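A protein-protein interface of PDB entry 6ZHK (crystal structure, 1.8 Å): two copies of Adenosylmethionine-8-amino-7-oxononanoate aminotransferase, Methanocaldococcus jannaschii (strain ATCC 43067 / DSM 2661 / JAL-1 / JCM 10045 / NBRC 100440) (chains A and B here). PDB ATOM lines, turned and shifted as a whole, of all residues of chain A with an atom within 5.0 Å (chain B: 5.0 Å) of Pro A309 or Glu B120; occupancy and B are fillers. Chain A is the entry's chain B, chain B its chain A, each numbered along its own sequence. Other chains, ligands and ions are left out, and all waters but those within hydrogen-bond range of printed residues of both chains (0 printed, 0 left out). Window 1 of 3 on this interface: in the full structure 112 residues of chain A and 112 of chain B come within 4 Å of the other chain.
OD2 of Asp B121 lies close to OE1 of Glu A120 (2.6 Å).
The side-chain hydroxyl (OH) of Tyr B339 sits close to the backbone carbonyl oxygen (O) of Leu A308 (3.4 Å).
The backbone carbonyl oxygen (O) of Tyr A307 lies within hydrogen-bond range of the side-chain amide nitrogen (ND2) of Asn B342, 3.0 Å away.
The side-chain hydroxyl (OH) of Tyr B339 sits at hydrogen-bond distance from the side-chain hydroxyl (OG1) of Thr A304 (3.4 Å).
Glu A120 touches Asp B121, but with the chains exchanged Asp A121 does not touch Glu B120 (4.5 Å).
Glu A120 touches Pro B309, and with the chains exchanged Pro A309 touches Glu B120.
O of Glu B120 sits at hydrogen-bond distance from N of Leu B310, 3.3 Å away.
OG1 of Thr A304 lies within hydrogen-bond range of N of Tyr A307 (3.4 Å).
The backbone NH of Glu B120 sits at hydrogen-bond distance from the side-chain carboxylate of Glu B124.
The backbone carbonyl oxygen (O) of Leu A308 lies within hydrogen-bond range of the side-chain hydroxyl (OG1) of Thr A304 (2.7 Å).
O of Glu A120 is in hydrogen-bond range of N of Leu A310 (3.3 Å).
The side-chain amide oxygen (OD1) of Asn B342 is in hydrogen-bond range of the backbone NH (N) of Leu B345, 2.9 Å away.
Of the 15 printed residues of chain B, 7 touch a printed residue of chain A.
Printed residues of chain B that touch a printed residue of chain A: Glu B120, Asp B121, Glu B124, Pro B309, His B337, Tyr B339 and Asn B342.
Hydrophobic or aromatic side chains of chain B that line the printed part of chain A: Pro B309, His B337 and Tyr B339.
Of the 10 printed residues of chain A, 6 touch a printed residue of chain B.
Hydrophobic or aromatic side chains of chain A within 4 Å of the printed part of chain B: Pro A309.
Along chain A the printed residues that touch a printed residue of chain B span positions 120 to 309.
Among the printed residues, no Asp or Glu carboxylate lies within 4 Å of a Lys or Arg side-chain nitrogen of the other chain.
Printed residues of chain B within 4 Å of Asp A121: Glu B124 (3.3 Å) and His B337 (3.5 Å).
Pro A309 touches two residues of chain B.
Of the printed residues of chain A, Glu B120 touches Pro A309 (3.9 Å).
Printed residues of chain A within 4 Å of His B337: Asp A121.
The nearest residue of chain B that does not touch Pro A309 is Pro B309 (4.02 Å).
The nearest printed residue of chain A that does not touch Asp B121 is Asp A121 (5.3 Å).
Pro B309 touches Glu A120.
Glu B124 touches Asp A121.
CB of Asp A121 touches CD2 of His B337 (3.5 Å).
Tyr A307 touches Tyr B339 (N to OH, 3.9 Å).
Glu B120 touches Pro A309.
Tyr B339 touches Pro A309.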
ATOM      1  N   SER A 119      -0.178 -13.318   0.386  1.00  0.00           N
ATOM      2  CA  SER A 119      -1.054 -14.224  -0.360  1.00  0.00           C
ATOM      3  C   SER A 119      -0.833 -15.626   0.187  1.00  0.00           C
ATOM      4  O   SER A 119      -0.130 -15.760   1.199  1.00  0.00           O
ATOM      5  CB  SER A 119      -0.819 -14.160  -1.853  1.00  0.00           C
ATOM      6  OG  SER A 119       0.532 -14.426  -2.182  1.00  0.00           O
ATOM      7  N   GLU A 120      -1.365 -16.658  -0.495  1.00  0.00           N
ATOM      8  CA  GLU A 120      -1.267 -18.011   0.044  1.00  0.00           C
ATOM      9  C   GLU A 120      -0.237 -18.866  -0.667  1.00  0.00           C
ATOM     10  O   GLU A 120       0.390 -19.692  -0.028  1.00  0.00           O
ATOM     11  CB  GLU A 120      -2.612 -18.756   0.010  1.00  0.00           C
ATOM     12  CG  GLU A 120      -3.552 -18.258   1.111  1.00  0.00           C
ATOM     13  CD  GLU A 120      -4.102 -16.858   0.858  1.00  0.00           C
ATOM     14  OE1 GLU A 120      -4.648 -16.629  -0.225  1.00  0.00           O
ATOM     15  OE2 GLU A 120      -3.963 -15.999   1.733  1.00  0.00           O
ATOM     16  N   ASP A 121      -0.012 -18.676  -1.979  1.00  0.00           N
ATOM     17  CA  ASP A 121       0.806 -19.616  -2.747  1.00  0.00           C
ATOM     18  C   ASP A 121       1.828 -18.785  -3.537  1.00  0.00           C
ATOM     19  O   ASP A 121       1.567 -17.604  -3.857  1.00  0.00           O
ATOM     20  CB  ASP A 121      -0.051 -20.335  -3.817  1.00  0.00           C
ATOM     21  N   THR A 304       6.518 -20.764   6.143  1.00  0.00           N
ATOM     22  CA  THR A 304       5.860 -21.297   7.323  1.00  0.00           C
ATOM     23  C   THR A 304       6.574 -22.541   7.849  1.00  0.00           C
ATOM     24  O   THR A 304       5.996 -23.311   8.641  1.00  0.00           O
ATOM     25  CB  THR A 304       4.420 -21.676   6.944  1.00  0.00           C
ATOM     26  OG1 THR A 304       4.605 -22.622   5.883  1.00  0.00           O
ATOM     27  CG2 THR A 304       3.644 -20.463   6.437  1.00  0.00           C
ATOM     28  N   TYR A 307       4.550 -25.851   6.893  1.00  0.00           N
ATOM     29  CA  TYR A 307       3.368 -26.419   7.541  1.00  0.00           C
ATOM     30  C   TYR A 307       2.047 -25.872   7.045  1.00  0.00           C
ATOM     31  O   TYR A 307       0.982 -26.551   7.181  1.00  0.00           O
ATOM     32  CB  TYR A 307       3.368 -26.279   9.075  1.00  0.00           C
ATOM     33  CG  TYR A 307       4.433 -27.096   9.767  1.00  0.00           C
ATOM     34  CD1 TYR A 307       5.276 -27.947   9.052  1.00  0.00           C
ATOM     35  CD2 TYR A 307       4.478 -27.154  11.152  1.00  0.00           C
ATOM     36  CE1 TYR A 307       6.267 -28.687   9.711  1.00  0.00           C
ATOM     37  CE2 TYR A 307       5.432 -27.913  11.817  1.00  0.00           C
ATOM     38  CZ  TYR A 307       6.303 -28.720  11.100  1.00  0.00           C
ATOM     39  OH  TYR A 307       7.222 -29.509  11.777  1.00  0.00           O
ATOM     40  N   LEU A 308       2.099 -24.660   6.470  1.00  0.00           N
ATOM     41  CA  LEU A 308       0.866 -24.035   5.966  1.00  0.00           C
ATOM     42  C   LEU A 308       1.156 -23.172   4.730  1.00  0.00           C
ATOM     43  O   LEU A 308       2.306 -22.746   4.503  1.00  0.00           O
ATOM     44  CB  LEU A 308       0.276 -23.148   7.066  1.00  0.00           C
ATOM     45  CG  LEU A 308      -0.609 -23.818   8.122  1.00  0.00           C
ATOM     46  CD1 LEU A 308      -0.851 -22.788   9.285  1.00  0.00           C
ATOM     47  CD2 LEU A 308      -1.954 -24.260   7.541  1.00  0.00           C
ATOM     48  N   PRO A 309       0.127 -22.861   3.914  1.00  0.00           N
ATOM     49  CA  PRO A 309       0.344 -22.067   2.699  1.00  0.00           C
ATOM     50  C   PRO A 309       0.295 -20.578   2.981  1.00  0.00           C
ATOM     51  O   PRO A 309      -0.758 -19.968   2.952  1.00  0.00           O
ATOM     52  CB  PRO A 309      -0.874 -22.392   1.829  1.00  0.00           C
ATOM     53  CG  PRO A 309      -1.959 -22.737   2.830  1.00  0.00           C
ATOM     54  CD  PRO A 309      -1.243 -23.446   3.949  1.00  0.00           C
ATOM     55  N   LEU A 310       1.483 -19.990   3.065  1.00  0.00           N
ATOM     56  CA  LEU A 310       1.605 -18.554   3.048  1.00  0.00           C
ATOM     57  C   LEU A 310       2.614 -18.147   1.973  1.00  0.00           C
ATOM     58  O   LEU A 310       3.657 -18.816   1.744  1.00  0.00           O
ATOM     59  CB  LEU A 310       2.082 -18.064   4.427  1.00  0.00           C
ATOM     60  CG  LEU A 310       2.132 -16.541   4.603  1.00  0.00           C
ATOM     61  CD1 LEU A 310       0.713 -15.970   4.480  1.00  0.00           C
ATOM     62  CD2 LEU A 310       2.715 -16.187   5.974  1.00  0.00           C
ATOM     63  N   ALA A 311       2.318 -17.008   1.349  1.00  0.00           N
ATOM     64  CA  ALA A 311       3.309 -16.411   0.480  1.00  0.00           C
ATOM     65  C   ALA A 311       3.313 -14.890   0.734  1.00  0.00           C
ATOM     66  O   ALA A 311       2.420 -14.337   1.340  1.00  0.00           O
ATOM     67  CB  ALA A 311       3.000 -16.800  -0.954  1.00  0.00           C
ATOM     68  N   LEU A 345      -1.766 -18.848   9.355  1.00  0.00           N
ATOM     69  CA  LEU A 345      -0.655 -18.879   8.420  1.00  0.00           C
ATOM     70  C   LEU A 345       0.470 -18.057   9.018  1.00  0.00           C
ATOM     71  O   LEU A 345       1.644 -18.463   8.978  1.00  0.00           O
ATOM     72  CB  LEU A 345      -1.024 -18.303   7.031  1.00  0.00           C
ATOM     73  CG  LEU A 345      -2.322 -18.822   6.395  1.00  0.00           C
ATOM     74  CD1 LEU A 345      -2.480 -18.276   4.959  1.00  0.00           C
ATOM     75  CD2 LEU A 345      -2.299 -20.368   6.313  1.00  0.00           C
ATOM     76  N   TYR B 118      -7.936 -30.199  -5.336  1.00  0.00           N
ATOM     77  CA  TYR B 118      -7.845 -29.212  -4.273  1.00  0.00           C
ATOM     78  C   TYR B 118      -6.917 -28.063  -4.646  1.00  0.00           C
ATOM     79  O   TYR B 118      -5.994 -28.231  -5.420  1.00  0.00           O
ATOM     80  CB  TYR B 118      -7.173 -29.832  -3.044  1.00  0.00           C
ATOM     81  CG  TYR B 118      -8.063 -30.838  -2.302  1.00  0.00           C
ATOM     82  CD1 TYR B 118      -9.191 -30.399  -1.616  1.00  0.00           C
ATOM     83  CD2 TYR B 118      -7.736 -32.200  -2.252  1.00  0.00           C
ATOM     84  CE1 TYR B 118      -9.975 -31.307  -0.896  1.00  0.00           C
ATOM     85  CE2 TYR B 118      -8.493 -33.104  -1.526  1.00  0.00           C
ATOM     86  CZ  TYR B 118      -9.633 -32.657  -0.880  1.00  0.00           C
ATOM     87  OH  TYR B 118     -10.414 -33.499  -0.139  1.00  0.00           O
ATOM     88  N   SER B 119      -7.159 -26.900  -4.030  1.00  0.00           N
ATOM     89  CA  SER B 119      -6.286 -25.740  -4.116  1.00  0.00           C
ATOM     90  C   SER B 119      -6.512 -24.920  -2.842  1.00  0.00           C
ATOM     91  O   SER B 119      -7.188 -25.395  -1.918  1.00  0.00           O
ATOM     92  CB  SER B 119      -6.549 -24.917  -5.373  1.00  0.00           C
ATOM     93  OG  SER B 119      -7.880 -24.438  -5.435  1.00  0.00           O
ATOM     94  N   GLU B 120      -5.970 -23.699  -2.789  1.00  0.00           N
ATOM     95  CA  GLU B 120      -6.031 -22.915  -1.563  1.00  0.00           C
ATOM     96  C   GLU B 120      -7.100 -21.833  -1.608  1.00  0.00           C
ATOM     97  O   GLU B 120      -7.730 -21.619  -0.601  1.00  0.00           O
ATOM     98  CB  GLU B 120      -4.684 -22.268  -1.235  1.00  0.00           C
ATOM     99  CG  GLU B 120      -3.703 -23.281  -0.679  1.00  0.00           C
ATOM    100  CD  GLU B 120      -3.185 -24.296  -1.677  1.00  0.00           C
ATOM    101  OE1 GLU B 120      -2.679 -23.856  -2.763  1.00  0.00           O
ATOM    102  OE2 GLU B 120      -3.368 -25.518  -1.399  1.00  0.00           O
ATOM    103  N   ASP B 121      -7.349 -21.201  -2.770  1.00  0.00           N
ATOM    104  CA  ASP B 121      -8.203 -20.011  -2.821  1.00  0.00           C
ATOM    105  C   ASP B 121      -9.208 -20.215  -3.951  1.00  0.00           C
ATOM    106  O   ASP B 121      -8.889 -20.912  -4.922  1.00  0.00           O
ATOM    107  CB  ASP B 121      -7.396 -18.745  -3.155  1.00  0.00           C
ATOM    108  CG  ASP B 121      -6.399 -18.438  -2.048  1.00  0.00           C
ATOM    109  OD1 ASP B 121      -6.727 -18.730  -0.873  1.00  0.00           O
ATOM    110  OD2 ASP B 121      -5.286 -17.910  -2.348  1.00  0.00           O
ATOM    111  N   GLY B 122     -10.379 -19.577  -3.823  1.00  0.00           N
ATOM    112  CA  GLY B 122     -11.431 -19.675  -4.829  1.00  0.00           C
ATOM    113  C   GLY B 122     -10.948 -19.188  -6.206  1.00  0.00           C
ATOM    114  O   GLY B 122     -11.351 -19.750  -7.232  1.00  0.00           O
ATOM    115  N   GLU B 124      -7.972 -19.601  -7.420  1.00  0.00           N
ATOM    116  CA  GLU B 124      -7.216 -20.711  -7.979  1.00  0.00           C
ATOM    117  C   GLU B 124      -8.176 -21.827  -8.434  1.00  0.00           C
ATOM    118  O   GLU B 124      -7.915 -22.467  -9.444  1.00  0.00           O
ATOM    119  CB  GLU B 124      -6.331 -21.317  -6.874  1.00  0.00           C
ATOM    120  CG  GLU B 124      -4.969 -20.660  -6.614  1.00  0.00           C
ATOM    121  CD  GLU B 124      -4.234 -21.051  -5.333  1.00  0.00           C
ATOM    122  OE1 GLU B 124      -4.794 -21.793  -4.508  1.00  0.00           O
ATOM    123  OE2 GLU B 124      -3.064 -20.617  -5.131  1.00  0.00           O
ATOM    124  N   PRO B 309      -7.473 -21.277   4.442  1.00  0.00           N
ATOM    125  CA  PRO B 309      -7.651 -21.219   2.991  1.00  0.00           C
ATOM    126  C   PRO B 309      -7.656 -22.614   2.385  1.00  0.00           C
ATOM    127  O   PRO B 309      -6.625 -23.138   1.979  1.00  0.00           O
ATOM    128  CB  PRO B 309      -6.448 -20.377   2.530  1.00  0.00           C
ATOM    129  CG  PRO B 309      -5.390 -20.738   3.472  1.00  0.00           C
ATOM    130  CD  PRO B 309      -6.096 -20.869   4.820  1.00  0.00           C
ATOM    131  N   LEU B 310      -8.866 -23.125   2.163  1.00  0.00           N
ATOM    132  CA  LEU B 310      -8.993 -24.282   1.282  1.00  0.00           C
ATOM    133  C   LEU B 310      -9.969 -23.998   0.145  1.00  0.00           C
ATOM    134  O   LEU B 310     -10.985 -23.341   0.348  1.00  0.00           O
ATOM    135  CB  LEU B 310      -9.454 -25.501   2.089  1.00  0.00           C
ATOM    136  CG  LEU B 310      -9.466 -26.820   1.306  1.00  0.00           C
ATOM    137  CD1 LEU B 310      -8.041 -27.172   0.858  1.00  0.00           C
ATOM    138  CD2 LEU B 310     -10.014 -27.926   2.210  1.00  0.00           C
ATOM    139  N   ALA B 311      -9.639 -24.488  -1.051  1.00  0.00           N
ATOM    140  CA  ALA B 311     -10.623 -24.454  -2.112  1.00  0.00           C
ATOM    141  C   ALA B 311     -10.644 -25.805  -2.827  1.00  0.00           C
ATOM    142  O   ALA B 311      -9.774 -26.653  -2.616  1.00  0.00           O
ATOM    143  CB  ALA B 311     -10.355 -23.296  -3.009  1.00  0.00           C
ATOM    144  N   HIS B 337      -0.219 -26.687  -6.844  1.00  0.00           N
ATOM    145  CA  HIS B 337       0.882 -26.073  -6.124  1.00  0.00           C
ATOM    146  C   HIS B 337       1.205 -26.885  -4.877  1.00  0.00           C
ATOM    147  O   HIS B 337       0.453 -27.807  -4.552  1.00  0.00           O
ATOM    148  CB  HIS B 337       0.664 -24.575  -5.876  1.00  0.00           C
ATOM    149  CG  HIS B 337       1.892 -23.705  -5.931  1.00  0.00           C
ATOM    150  ND1 HIS B 337       3.168 -24.207  -6.075  1.00  0.00           N
ATOM    151  CD2 HIS B 337       2.028 -22.366  -5.836  1.00  0.00           C
ATOM    152  CE1 HIS B 337       4.036 -23.222  -6.080  1.00  0.00           C
ATOM    153  NE2 HIS B 337       3.360 -22.093  -5.920  1.00  0.00           N
ATOM    154  N   TYR B 339       0.946 -26.789  -1.713  1.00  0.00           N
ATOM    155  CA  TYR B 339       0.224 -27.116  -0.474  1.00  0.00           C
ATOM    156  C   TYR B 339      -1.104 -27.765  -0.856  1.00  0.00           C
ATOM    157  O   TYR B 339      -1.970 -27.931   0.019  1.00  0.00           O
ATOM    158  CB  TYR B 339       0.061 -25.839   0.376  1.00  0.00           C
ATOM    159  CG  TYR B 339       1.332 -25.498   1.141  1.00  0.00           C
ATOM    160  CD1 TYR B 339       1.709 -26.270   2.251  1.00  0.00           C
ATOM    161  CD2 TYR B 339       2.169 -24.462   0.727  1.00  0.00           C
ATOM    162  CE1 TYR B 339       2.924 -26.032   2.908  1.00  0.00           C
ATOM    163  CE2 TYR B 339       3.320 -24.164   1.426  1.00  0.00           C
ATOM    164  CZ  TYR B 339       3.678 -24.944   2.520  1.00  0.00           C
ATOM    165  OH  TYR B 339       4.812 -24.650   3.216  1.00  0.00           O
ATOM    166  N   THR B 340      -1.193 -28.282  -2.094  1.00  0.00           N
ATOM    167  CA  THR B 340      -2.474 -28.935  -2.504  1.00  0.00           C
ATOM    168  C   THR B 340      -2.829 -30.046  -1.486  1.00  0.00           C
ATOM    169  O   THR B 340      -2.017 -30.937  -1.183  1.00  0.00           O
ATOM    170  CB  THR B 340      -2.263 -29.625  -3.879  1.00  0.00           C
ATOM    171  OG1 THR B 340      -1.981 -28.579  -4.833  1.00  0.00           O
ATOM    172  CG2 THR B 340      -3.505 -30.366  -4.369  1.00  0.00           C
ATOM    173  N   GLY B 341      -4.065 -30.079  -1.022  1.00  0.00           N
ATOM    174  CA  GLY B 341      -4.520 -31.076  -0.044  1.00  0.00           C
ATOM    175  C   GLY B 341      -3.862 -31.022   1.345  1.00  0.00           C
ATOM    176  O   GLY B 341      -3.845 -32.030   2.080  1.00  0.00           O
ATOM    177  N   ASN B 342      -3.342 -29.868   1.782  1.00  0.00           N
ATOM    178  CA  ASN B 342      -2.640 -29.762   3.064  1.00  0.00           C
ATOM    179  C   ASN B 342      -3.512 -30.304   4.230  1.00  0.00           C
ATOM    180  O   ASN B 342      -4.712 -30.031   4.299  1.00  0.00           O
ATOM    181  CB  ASN B 342      -2.323 -28.268   3.294  1.00  0.00           C
ATOM    182  CG  ASN B 342      -1.920 -27.970   4.714  1.00  0.00           C
ATOM    183  OD1 ASN B 342      -2.737 -27.821   5.593  1.00  0.00           O
ATOM    184  ND2 ASN B 342      -0.640 -27.708   4.899  1.00  0.00           N
ATOM    185  N   LEU B 345      -5.541 -27.763   6.412  1.00  0.00           N
ATOM    186  CA  LEU B 345      -6.666 -27.178   5.695  1.00  0.00           C
ATOM    187  C   LEU B 345      -7.784 -28.203   5.694  1.00  0.00           C
ATOM    188  O   LEU B 345      -8.936 -27.849   5.917  1.00  0.00           O
ATOM    189  CB  LEU B 345      -6.333 -26.821   4.222  1.00  0.00           C
ATOM    190  CG  LEU B 345      -5.025 -26.048   4.024  1.00  0.00           C
ATOM    191  CD1 LEU B 345      -4.833 -25.602   2.579  1.00  0.00           C
ATOM    192  CD2 LEU B 345      -5.005 -24.794   4.885  1.00  0.00           C
